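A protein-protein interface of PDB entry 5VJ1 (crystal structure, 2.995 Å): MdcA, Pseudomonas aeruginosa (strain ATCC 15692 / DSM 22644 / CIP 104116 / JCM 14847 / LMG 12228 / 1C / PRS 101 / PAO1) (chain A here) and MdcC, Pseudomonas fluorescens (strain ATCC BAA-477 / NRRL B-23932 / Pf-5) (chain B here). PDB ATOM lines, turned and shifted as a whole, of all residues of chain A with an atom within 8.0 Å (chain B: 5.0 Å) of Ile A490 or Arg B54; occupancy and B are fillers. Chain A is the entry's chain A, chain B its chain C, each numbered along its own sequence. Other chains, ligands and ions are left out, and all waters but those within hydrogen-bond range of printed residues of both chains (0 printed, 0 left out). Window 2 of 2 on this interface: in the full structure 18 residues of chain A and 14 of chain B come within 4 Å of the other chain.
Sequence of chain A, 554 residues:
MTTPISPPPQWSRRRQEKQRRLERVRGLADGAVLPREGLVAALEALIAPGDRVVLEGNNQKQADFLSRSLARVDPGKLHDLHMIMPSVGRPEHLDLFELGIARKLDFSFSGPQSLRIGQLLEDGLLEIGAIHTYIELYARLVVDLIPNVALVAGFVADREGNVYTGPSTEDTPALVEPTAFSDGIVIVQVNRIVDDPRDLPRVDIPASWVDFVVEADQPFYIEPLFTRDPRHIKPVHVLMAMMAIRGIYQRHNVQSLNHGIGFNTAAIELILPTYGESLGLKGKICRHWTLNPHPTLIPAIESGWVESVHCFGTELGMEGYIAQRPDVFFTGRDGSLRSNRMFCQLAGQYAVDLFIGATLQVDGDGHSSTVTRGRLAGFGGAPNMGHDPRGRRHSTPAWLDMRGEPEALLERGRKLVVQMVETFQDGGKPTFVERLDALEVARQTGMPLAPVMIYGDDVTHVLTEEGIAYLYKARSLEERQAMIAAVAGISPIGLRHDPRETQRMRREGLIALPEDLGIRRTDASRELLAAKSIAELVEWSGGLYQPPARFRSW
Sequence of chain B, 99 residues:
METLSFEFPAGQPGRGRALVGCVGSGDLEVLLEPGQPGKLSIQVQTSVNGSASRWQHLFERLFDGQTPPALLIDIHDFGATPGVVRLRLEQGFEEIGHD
O of Gly A428 is in hydrogen-bond range of NH2 of Arg B54. The backbone carbonyl oxygen (O) of Gly A489 is in hydrogen-bond range of the guanidinium group (NH1) of Arg B61. The guanidinium group of Arg B61 is in hydrogen-bond range of the backbone carbonyl oxygen of Gly A494 (3.0 Å).
The side-chain hydroxyl of Ser A491 is in hydrogen-bond range of the backbone NH of Gly A494, at 3.3 Å.
Among the printed residues, merely in contact across the chains: Phe A424 with Arg B54 (3.6 Å), Phe A424 with Pro B82 (3.4 Å), Ile A490 with Arg B54 (3.6 Å), Ile A490 with His B57 (3.8 Å), Ile A490 with Arg B61 (3.9 Å), Ile A490 with Pro B82 (3.6 Å) and Leu A495 with His B57 (3.9 Å).
Arg B54 touches just these residues of chain A: Phe A424, Gly A428 and Ile A490. No residue of chain A comes within 4 Å of Ser B53. Of the printed residues of chain B, Gly A489 touches Arg B61 (3.1 Å). Of the printed residues of chain B, Gly A494 touches Arg B61 (3.0 Å). Printed residues of chain A within 4 Å of Pro B82: Phe A424 (3.4 Å) and Ile A490 (3.6 Å). Of the printed residues of chain A, Arg B61 touches Gly A489 (3.1 Å), Ile A490 (3.9 Å) and Gly A494 (3.0 Å). The nearest residue of chain B that does not touch Ile A490 is Leu B58 (4.02 Å). The nearest residue of chain A that does not touch Arg B54 is Pro A430 (4.9 Å). The nearest printed residue of chain B that does not touch Gly A489 is Pro B82 (6.9 Å).
Of the 23 printed residues of chain A, 6 touch a printed residue of chain B. Hydrophobic or aromatic side chains of chain B within 4 Å of the printed part of chain A: His B57 and Pro B82. Among the printed residues, 10 pairs touch across the chains. Among the printed residues, no Asp or Glu carboxylate lies within 4 Å of a Lys or Arg side-chain nitrogen of the other chain.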
ATOM      1  N   THR A 423     -11.832 -10.161  13.214  1.00  0.00           N
ATOM      2  CA  THR A 423     -10.911  -9.897  14.312  1.00  0.00           C
ATOM      3  C   THR A 423     -10.848 -11.065  15.249  1.00  0.00           C
ATOM      4  O   THR A 423      -9.856 -11.248  15.953  1.00  0.00           O
ATOM      5  CB  THR A 423     -11.322  -8.687  15.096  1.00  0.00           C
ATOM      6  OG1 THR A 423     -12.742  -8.747  15.295  1.00  0.00           O
ATOM      7  CG2 THR A 423     -10.987  -7.461  14.325  1.00  0.00           C
ATOM      8  N   PHE A 424     -11.915 -11.864  15.248  1.00  0.00           N
ATOM      9  CA  PHE A 424     -11.978 -13.032  16.118  1.00  0.00           C
ATOM     10  C   PHE A 424     -12.399 -14.306  15.419  1.00  0.00           C
ATOM     11  O   PHE A 424     -13.335 -14.356  14.615  1.00  0.00           O
ATOM     12  CB  PHE A 424     -12.921 -12.794  17.293  1.00  0.00           C
ATOM     13  CG  PHE A 424     -12.306 -12.021  18.412  1.00  0.00           C
ATOM     14  CD1 PHE A 424     -12.173 -10.657  18.306  1.00  0.00           C
ATOM     15  CD2 PHE A 424     -11.855 -12.651  19.560  1.00  0.00           C
ATOM     16  CE1 PHE A 424     -11.628  -9.933  19.315  1.00  0.00           C
ATOM     17  CE2 PHE A 424     -11.296 -11.923  20.576  1.00  0.00           C
ATOM     18  CZ  PHE A 424     -11.183 -10.561  20.453  1.00  0.00           C
ATOM     19  N   GLY A 427     -14.612 -19.302  18.290  1.00  0.00           N
ATOM     20  CA  GLY A 427     -14.424 -19.794  19.643  1.00  0.00           C
ATOM     21  C   GLY A 427     -13.892 -18.850  20.707  1.00  0.00           C
ATOM     22  O   GLY A 427     -13.333 -19.323  21.708  1.00  0.00           O
ATOM     23  N   GLY A 428     -14.128 -17.544  20.541  1.00  0.00           N
ATOM     24  CA  GLY A 428     -13.688 -16.519  21.485  1.00  0.00           C
ATOM     25  C   GLY A 428     -12.176 -16.275  21.556  1.00  0.00           C
ATOM     26  O   GLY A 428     -11.710 -15.443  22.360  1.00  0.00           O
ATOM     27  N   LYS A 429     -11.416 -16.996  20.718  1.00  0.00           N
ATOM     28  CA  LYS A 429      -9.983 -16.742  20.534  1.00  0.00           C
ATOM     29  C   LYS A 429      -9.863 -15.526  19.619  1.00  0.00           C
ATOM     30  O   LYS A 429     -10.652 -15.361  18.688  1.00  0.00           O
ATOM     31  CB  LYS A 429      -9.242 -17.957  19.939  1.00  0.00           C
ATOM     32  CG  LYS A 429      -8.744 -18.934  21.010  1.00  0.00           C
ATOM     33  CD  LYS A 429      -8.602 -20.377  20.520  1.00  0.00           C
ATOM     34  CE  LYS A 429      -8.342 -21.384  21.687  1.00  0.00           C
ATOM     35  NZ  LYS A 429      -7.419 -20.949  22.787  1.00  0.00           N
ATOM     36  N   PRO A 430      -8.885 -14.656  19.883  1.00  0.00           N
ATOM     37  CA  PRO A 430      -8.629 -13.556  18.947  1.00  0.00           C
ATOM     38  C   PRO A 430      -7.814 -14.015  17.715  1.00  0.00           C
ATOM     39  O   PRO A 430      -7.037 -14.965  17.828  1.00  0.00           O
ATOM     40  CB  PRO A 430      -7.843 -12.572  19.811  1.00  0.00           C
ATOM     41  CG  PRO A 430      -7.119 -13.468  20.774  1.00  0.00           C
ATOM     42  CD  PRO A 430      -8.121 -14.506  21.131  1.00  0.00           C
ATOM     43  N   THR A 431      -8.012 -13.399  16.553  1.00  0.00           N
ATOM     44  CA  THR A 431      -7.222 -13.785  15.391  1.00  0.00           C
ATOM     45  C   THR A 431      -5.844 -13.125  15.437  1.00  0.00           C
ATOM     46  O   THR A 431      -4.816 -13.773  15.211  1.00  0.00           O
ATOM     47  CB  THR A 431      -7.909 -13.430  14.057  1.00  0.00           C
ATOM     48  OG1 THR A 431      -9.099 -14.210  13.897  1.00  0.00           O
ATOM     49  CG2 THR A 431      -6.980 -13.761  12.907  1.00  0.00           C
ATOM     50  N   PHE A 432      -5.837 -11.824  15.697  1.00  0.00           N
ATOM     51  CA  PHE A 432      -4.601 -11.068  15.802  1.00  0.00           C
ATOM     52  C   PHE A 432      -4.013 -11.173  17.216  1.00  0.00           C
ATOM     53  O   PHE A 432      -4.490 -10.542  18.159  1.00  0.00           O
ATOM     54  CB  PHE A 432      -4.845  -9.611  15.394  1.00  0.00           C
ATOM     55  CG  PHE A 432      -5.320  -9.453  13.969  1.00  0.00           C
ATOM     56  CD1 PHE A 432      -6.669  -9.374  13.668  1.00  0.00           C
ATOM     57  CD2 PHE A 432      -4.407  -9.389  12.923  1.00  0.00           C
ATOM     58  CE1 PHE A 432      -7.100  -9.227  12.347  1.00  0.00           C
ATOM     59  CE2 PHE A 432      -4.831  -9.238  11.596  1.00  0.00           C
ATOM     60  CZ  PHE A 432      -6.176  -9.159  11.313  1.00  0.00           C
ATOM     61  N   THR A 464     -10.690  -6.716   7.421  1.00  0.00           N
ATOM     62  CA  THR A 464     -11.343  -7.056   8.678  1.00  0.00           C
ATOM     63  C   THR A 464     -12.762  -6.482   8.710  1.00  0.00           C
ATOM     64  O   THR A 464     -13.034  -5.531   7.985  1.00  0.00           O
ATOM     65  CB  THR A 464     -10.484  -6.508   9.846  1.00  0.00           C
ATOM     66  OG1 THR A 464      -9.319  -7.334  10.002  1.00  0.00           O
ATOM     67  CG2 THR A 464     -11.217  -6.515  11.106  1.00  0.00           C
ATOM     68  N   GLU A 465     -13.659  -7.002   9.556  1.00  0.00           N
ATOM     69  CA  GLU A 465     -14.969  -6.364   9.721  1.00  0.00           C
ATOM     70  C   GLU A 465     -14.786  -4.927  10.272  1.00  0.00           C
ATOM     71  O   GLU A 465     -15.709  -4.122  10.269  1.00  0.00           O
ATOM     72  CB  GLU A 465     -15.885  -7.176  10.657  1.00  0.00           C
ATOM     73  CG  GLU A 465     -15.701  -6.861  12.156  1.00  0.00           C
ATOM     74  CD  GLU A 465     -14.559  -7.638  12.814  1.00  0.00           C
ATOM     75  OE1 GLU A 465     -13.750  -8.244  12.080  1.00  0.00           O
ATOM     76  OE2 GLU A 465     -14.445  -7.606  14.064  1.00  0.00           O
ATOM     77  N   GLU A 466     -13.565  -4.579  10.648  1.00  0.00           N
ATOM     78  CA  GLU A 466     -13.286  -3.274  11.201  1.00  0.00           C
ATOM     79  C   GLU A 466     -13.005  -2.316  10.100  1.00  0.00           C
ATOM     80  O   GLU A 466     -13.330  -1.149  10.220  1.00  0.00           O
ATOM     81  CB  GLU A 466     -12.080  -3.304  12.128  1.00  0.00           C
ATOM     82  CG  GLU A 466     -12.339  -3.894  13.492  1.00  0.00           C
ATOM     83  CD  GLU A 466     -13.011  -2.903  14.403  1.00  0.00           C
ATOM     84  OE1 GLU A 466     -12.304  -1.956  14.834  1.00  0.00           O
ATOM     85  OE2 GLU A 466     -14.233  -3.081  14.676  1.00  0.00           O
ATOM     86  N   ALA A 485      -2.905  -2.942  13.700  1.00  0.00           N
ATOM     87  CA  ALA A 485      -3.617  -2.744  14.957  1.00  0.00           C
ATOM     88  C   ALA A 485      -4.872  -1.882  14.780  1.00  0.00           C
ATOM     89  O   ALA A 485      -5.841  -2.059  15.505  1.00  0.00           O
ATOM     90  CB  ALA A 485      -2.702  -2.135  15.980  1.00  0.00           C
ATOM     91  N   ALA A 486      -4.857  -0.947  13.834  1.00  0.00           N
ATOM     92  CA  ALA A 486      -6.014  -0.080  13.580  1.00  0.00           C
ATOM     93  C   ALA A 486      -7.247  -0.869  13.104  1.00  0.00           C
ATOM     94  O   ALA A 486      -8.373  -0.543  13.450  1.00  0.00           O
ATOM     95  CB  ALA A 486      -5.662   0.996  12.592  1.00  0.00           C
ATOM     96  N   VAL A 487      -7.052  -1.873  12.271  1.00  0.00           N
ATOM     97  CA  VAL A 487      -8.179  -2.695  11.847  1.00  0.00           C
ATOM     98  C   VAL A 487      -8.372  -3.948  12.709  1.00  0.00           C
ATOM     99  O   VAL A 487      -9.239  -4.770  12.421  1.00  0.00           O
ATOM    100  CB  VAL A 487      -8.021  -3.150  10.392  1.00  0.00           C
ATOM    101  CG1 VAL A 487      -7.616  -1.965   9.525  1.00  0.00           C
ATOM    102  CG2 VAL A 487      -6.994  -4.293  10.297  1.00  0.00           C
ATOM    103  N   ALA A 488      -7.567  -4.100  13.758  1.00  0.00           N
ATOM    104  CA  ALA A 488      -7.528  -5.359  14.520  1.00  0.00           C
ATOM    105  C   ALA A 488      -8.560  -5.476  15.655  1.00  0.00           C
ATOM    106  O   ALA A 488      -8.562  -6.464  16.391  1.00  0.00           O
ATOM    107  CB  ALA A 488      -6.124  -5.580  15.071  1.00  0.00           C
ATOM    108  N   GLY A 489      -9.432  -4.483  15.804  1.00  0.00           N
ATOM    109  CA  GLY A 489     -10.541  -4.619  16.735  1.00  0.00           C
ATOM    110  C   GLY A 489     -10.117  -4.636  18.183  1.00  0.00           C
ATOM    111  O   GLY A 489      -9.234  -3.875  18.577  1.00  0.00           O
ATOM    112  N   ILE A 490     -10.783  -5.453  18.994  1.00  0.00           N
ATOM    113  CA  ILE A 490     -10.410  -5.536  20.407  1.00  0.00           C
ATOM    114  C   ILE A 490      -9.584  -6.795  20.724  1.00  0.00           C
ATOM    115  O   ILE A 490      -9.583  -7.289  21.855  1.00  0.00           O
ATOM    116  CB  ILE A 490     -11.649  -5.480  21.332  1.00  0.00           C
ATOM    117  CG1 ILE A 490     -12.638  -6.588  20.978  1.00  0.00           C
ATOM    118  CG2 ILE A 490     -12.281  -4.097  21.287  1.00  0.00           C
ATOM    119  CD1 ILE A 490     -13.820  -6.619  21.866  1.00  0.00           C
ATOM    120  N   SER A 491      -8.859  -7.285  19.722  1.00  0.00           N
ATOM    121  CA  SER A 491      -7.895  -8.367  19.904  1.00  0.00           C
ATOM    122  C   SER A 491      -6.686  -7.783  20.616  1.00  0.00           C
ATOM    123  O   SER A 491      -6.511  -6.565  20.639  1.00  0.00           O
ATOM    124  CB  SER A 491      -7.487  -8.972  18.557  1.00  0.00           C
ATOM    125  OG  SER A 491      -6.810  -8.021  17.738  1.00  0.00           O
ATOM    126  N   PRO A 492      -5.862  -8.632  21.235  1.00  0.00           N
ATOM    127  CA  PRO A 492      -4.687  -8.094  21.922  1.00  0.00           C
ATOM    128  C   PRO A 492      -3.781  -7.221  21.029  1.00  0.00           C
ATOM    129  O   PRO A 492      -3.124  -6.328  21.541  1.00  0.00           O
ATOM    130  CB  PRO A 492      -3.979  -9.358  22.413  1.00  0.00           C
ATOM    131  CG  PRO A 492      -4.564 -10.475  21.602  1.00  0.00           C
ATOM    132  CD  PRO A 492      -5.966 -10.085  21.408  1.00  0.00           C
ATOM    133  N   ILE A 493      -3.770  -7.451  19.720  1.00  0.00           N
ATOM    134  CA  ILE A 493      -2.983  -6.620  18.806  1.00  0.00           C
ATOM    135  C   ILE A 493      -3.699  -5.292  18.633  1.00  0.00           C
ATOM    136  O   ILE A 493      -3.080  -4.228  18.674  1.00  0.00           O
ATOM    137  CB  ILE A 493      -2.763  -7.310  17.417  1.00  0.00           C
ATOM    138  CG1 ILE A 493      -1.672  -8.376  17.511  1.00  0.00           C
ATOM    139  CG2 ILE A 493      -2.439  -6.302  16.325  1.00  0.00           C
ATOM    140  CD1 ILE A 493      -0.369  -7.822  17.922  1.00  0.00           C
ATOM    141  N   GLY A 494      -5.019  -5.357  18.475  1.00  0.00           N
ATOM    142  CA  GLY A 494      -5.812  -4.162  18.251  1.00  0.00           C
ATOM    143  C   GLY A 494      -5.913  -3.251  19.455  1.00  0.00           C
ATOM    144  O   GLY A 494      -6.180  -2.064  19.318  1.00  0.00           O
ATOM    145  N   LEU A 495      -5.671  -3.797  20.641  1.00  0.00           N
ATOM    146  CA  LEU A 495      -5.692  -2.997  21.860  1.00  0.00           C
ATOM    147  C   LEU A 495      -4.417  -2.162  21.983  1.00  0.00           C
ATOM    148  O   LEU A 495      -4.312  -1.340  22.890  1.00  0.00           O
ATOM    149  CB  LEU A 495      -5.846  -3.886  23.078  1.00  0.00           C
ATOM    150  CG  LEU A 495      -7.191  -4.561  23.268  1.00  0.00           C
ATOM    151  CD1 LEU A 495      -7.057  -5.627  24.341  1.00  0.00           C
ATOM    152  CD2 LEU A 495      -8.248  -3.544  23.630  1.00  0.00           C
ATOM    153  N   ARG A 496      -3.450  -2.388  21.089  1.00  0.00           N
ATOM    154  CA  ARG A 496      -2.252  -1.552  21.017  1.00  0.00           C
ATOM    155  C   ARG A 496      -2.578  -0.213  20.345  1.00  0.00           C
ATOM    156  O   ARG A 496      -1.926   0.811  20.565  1.00  0.00           O
ATOM    157  CB  ARG A 496      -1.144  -2.248  20.236  1.00  0.00           C
ATOM    158  CG  ARG A 496      -0.624  -3.532  20.843  1.00  0.00           C
ATOM    159  CD  ARG A 496       0.552  -4.052  20.031  1.00  0.00           C
ATOM    160  NE  ARG A 496       1.008  -5.373  20.460  1.00  0.00           N
ATOM    161  CZ  ARG A 496       1.866  -6.115  19.763  1.00  0.00           C
ATOM    162  NH1 ARG A 496       2.357  -5.664  18.603  1.00  0.00           N
ATOM    163  NH2 ARG A 496       2.229  -7.313  20.214  1.00  0.00           N
ATOM    164  N   GLY B  50     -15.460 -15.196  31.684  1.00  0.00           N
ATOM    165  CA  GLY B  50     -14.348 -14.269  31.823  1.00  0.00           C
ATOM    166  C   GLY B  50     -14.136 -13.357  30.636  1.00  0.00           C
ATOM    167  O   GLY B  50     -13.006 -12.963  30.332  1.00  0.00           O
ATOM    168  N   SER B  51     -15.226 -13.019  29.961  1.00  0.00           N
ATOM    169  CA  SER B  51     -15.159 -12.111  28.826  1.00  0.00           C
ATOM    170  C   SER B  51     -15.401 -10.667  29.249  1.00  0.00           C
ATOM    171  O   SER B  51     -15.187  -9.766  28.465  1.00  0.00           O
ATOM    172  CB  SER B  51     -16.154 -12.526  27.746  1.00  0.00           C
ATOM    173  OG  SER B  51     -17.439 -12.707  28.303  1.00  0.00           O
ATOM    174  N   ALA B  52     -15.856 -10.460  30.481  1.00  0.00           N
ATOM    175  CA  ALA B  52     -16.141  -9.124  31.024  1.00  0.00           C
ATOM    176  C   ALA B  52     -15.234  -7.990  30.517  1.00  0.00           C
ATOM    177  O   ALA B  52     -15.721  -6.955  30.071  1.00  0.00           O
ATOM    178  CB  ALA B  52     -16.103  -9.176  32.547  1.00  0.00           C
ATOM    179  N   SER B  53     -13.920  -8.185  30.578  1.00  0.00           N
ATOM    180  CA  SER B  53     -12.968  -7.162  30.114  1.00  0.00           C
ATOM    181  C   SER B  53     -13.123  -6.892  28.621  1.00  0.00           C
ATOM    182  O   SER B  53     -13.003  -5.747  28.165  1.00  0.00           O
ATOM    183  CB  SER B  53     -11.530  -7.584  30.436  1.00  0.00           C
ATOM    184  OG  SER B  53     -11.356  -8.975  30.209  1.00  0.00           O
ATOM    185  N   ARG B  54     -13.380  -7.962  27.870  1.00  0.00           N
ATOM    186  CA  ARG B  54     -13.607  -7.886  26.436  1.00  0.00           C
ATOM    187  C   ARG B  54     -14.860  -7.047  26.119  1.00  0.00           C
ATOM    188  O   ARG B  54     -14.805  -6.120  25.301  1.00  0.00           O
ATOM    189  CB  ARG B  54     -13.708  -9.304  25.884  1.00  0.00           C
ATOM    190  CG  ARG B  54     -13.666  -9.430  24.394  1.00  0.00           C
ATOM    191  CD  ARG B  54     -13.954 -10.861  23.939  1.00  0.00           C
ATOM    192  NE  ARG B  54     -12.719 -11.646  23.887  1.00  0.00           N
ATOM    193  CZ  ARG B  54     -12.200 -12.327  24.905  1.00  0.00           C
ATOM    194  NH1 ARG B  54     -12.866 -12.414  26.053  1.00  0.00           N
ATOM    195  NH2 ARG B  54     -11.051 -12.986  24.743  1.00  0.00           N
ATOM    196  N   TRP B  55     -15.973  -7.333  26.796  1.00  0.00           N
ATOM    197  CA  TRP B  55     -17.204  -6.549  26.626  1.00  0.00           C
ATOM    198  C   TRP B  55     -16.963  -5.087  26.998  1.00  0.00           C
ATOM    199  O   TRP B  55     -17.529  -4.184  26.385  1.00  0.00           O
ATOM    200  CB  TRP B  55     -18.359  -7.125  27.461  1.00  0.00           C
ATOM    201  CG  TRP B  55     -18.929  -8.381  26.880  1.00  0.00           C
ATOM    202  CD1 TRP B  55     -18.540  -9.662  27.156  1.00  0.00           C
ATOM    203  CD2 TRP B  55     -19.979  -8.484  25.915  1.00  0.00           C
ATOM    204  NE1 TRP B  55     -19.276 -10.558  26.419  1.00  0.00           N
ATOM    205  CE2 TRP B  55     -20.168  -9.859  25.644  1.00  0.00           C
ATOM    206  CE3 TRP B  55     -20.769  -7.550  25.236  1.00  0.00           C
ATOM    207  CZ2 TRP B  55     -21.130 -10.321  24.738  1.00  0.00           C
ATOM    208  CZ3 TRP B  55     -21.718  -8.007  24.336  1.00  0.00           C
ATOM    209  CH2 TRP B  55     -21.894  -9.378  24.099  1.00  0.00           C
ATOM    210  N   GLN B  56     -16.111  -4.850  27.991  1.00  0.00           N
ATOM    211  CA  GLN B  56     -15.809  -3.481  28.402  1.00  0.00           C
ATOM    212  C   GLN B  56     -15.243  -2.664  27.233  1.00  0.00           C
ATOM    213  O   GLN B  56     -15.767  -1.589  26.905  1.00  0.00           O
ATOM    214  CB  GLN B  56     -14.823  -3.477  29.572  1.00  0.00           C
ATOM    215  CG  GLN B  56     -14.529  -2.106  30.175  1.00  0.00           C
ATOM    216  CD  GLN B  56     -15.752  -1.467  30.791  1.00  0.00           C
ATOM    217  OE1 GLN B  56     -16.097  -0.327  30.476  1.00  0.00           O
ATOM    218  NE2 GLN B  56     -16.425  -2.205  31.674  1.00  0.00           N
ATOM    219  N   HIS B  57     -14.189  -3.196  26.607  1.00  0.00           N
ATOM    220  CA  HIS B  57     -13.530  -2.527  25.491  1.00  0.00           C
ATOM    221  C   HIS B  57     -14.473  -2.324  24.330  1.00  0.00           C
ATOM    222  O   HIS B  57     -14.482  -1.253  23.709  1.00  0.00           O
ATOM    223  CB  HIS B  57     -12.314  -3.310  25.024  1.00  0.00           C
ATOM    224  CG  HIS B  57     -11.245  -3.428  26.054  1.00  0.00           C
ATOM    225  ND1 HIS B  57     -10.707  -2.322  26.681  1.00  0.00           N
ATOM    226  CD2 HIS B  57     -10.600  -4.503  26.564  1.00  0.00           C
ATOM    227  CE1 HIS B  57      -9.785  -2.722  27.549  1.00  0.00           C
ATOM    228  NE2 HIS B  57      -9.703  -4.036  27.490  1.00  0.00           N
ATOM    229  N   LEU B  58     -15.264  -3.353  24.034  1.00  0.00           N
ATOM    230  CA  LEU B  58     -16.225  -3.251  22.955  1.00  0.00           C
ATOM    231  C   LEU B  58     -17.081  -2.012  23.156  1.00  0.00           C
ATOM    232  O   LEU B  58     -17.195  -1.181  22.263  1.00  0.00           O
ATOM    233  CB  LEU B  58     -17.088  -4.505  22.882  1.00  0.00           C
ATOM    234  CG  LEU B  58     -17.975  -4.571  21.639  1.00  0.00           C
ATOM    235  CD1 LEU B  58     -17.176  -4.214  20.376  1.00  0.00           C
ATOM    236  CD2 LEU B  58     -18.515  -5.966  21.519  1.00  0.00           C
ATOM    237  N   ARG B  61     -15.392   1.632  23.090  1.00  0.00           N
ATOM    238  CA  ARG B  61     -15.115   2.006  21.703  1.00  0.00           C
ATOM    239  C   ARG B  61     -16.392   2.460  21.010  1.00  0.00           C
ATOM    240  O   ARG B  61     -16.401   3.471  20.304  1.00  0.00           O
ATOM    241  CB  ARG B  61     -14.471   0.839  20.958  1.00  0.00           C
ATOM    242  CG  ARG B  61     -13.053   0.548  21.414  1.00  0.00           C
ATOM    243  CD  ARG B  61     -12.334  -0.275  20.408  1.00  0.00           C
ATOM    244  NE  ARG B  61     -10.892  -0.235  20.606  1.00  0.00           N
ATOM    245  CZ  ARG B  61     -10.013  -0.614  19.679  1.00  0.00           C
ATOM    246  NH1 ARG B  61     -10.445  -1.043  18.493  1.00  0.00           N
ATOM    247  NH2 ARG B  61      -8.704  -0.548  19.926  1.00  0.00           N
ATOM    248  N   PRO B  82     -16.767 -10.628  18.893  1.00  0.00           N
ATOM    249  CA  PRO B  82     -16.812  -9.171  19.091  1.00  0.00           C
ATOM    250  C   PRO B  82     -17.201  -8.421  17.801  1.00  0.00           C
ATOM    251  O   PRO B  82     -17.798  -7.340  17.867  1.00  0.00           O
ATOM    252  CB  PRO B  82     -15.388  -8.843  19.506  1.00  0.00           C
ATOM    253  CG  PRO B  82     -14.936 -10.060  20.192  1.00  0.00           C
ATOM    254  CD  PRO B  82     -15.507 -11.193  19.405  1.00  0.00           C
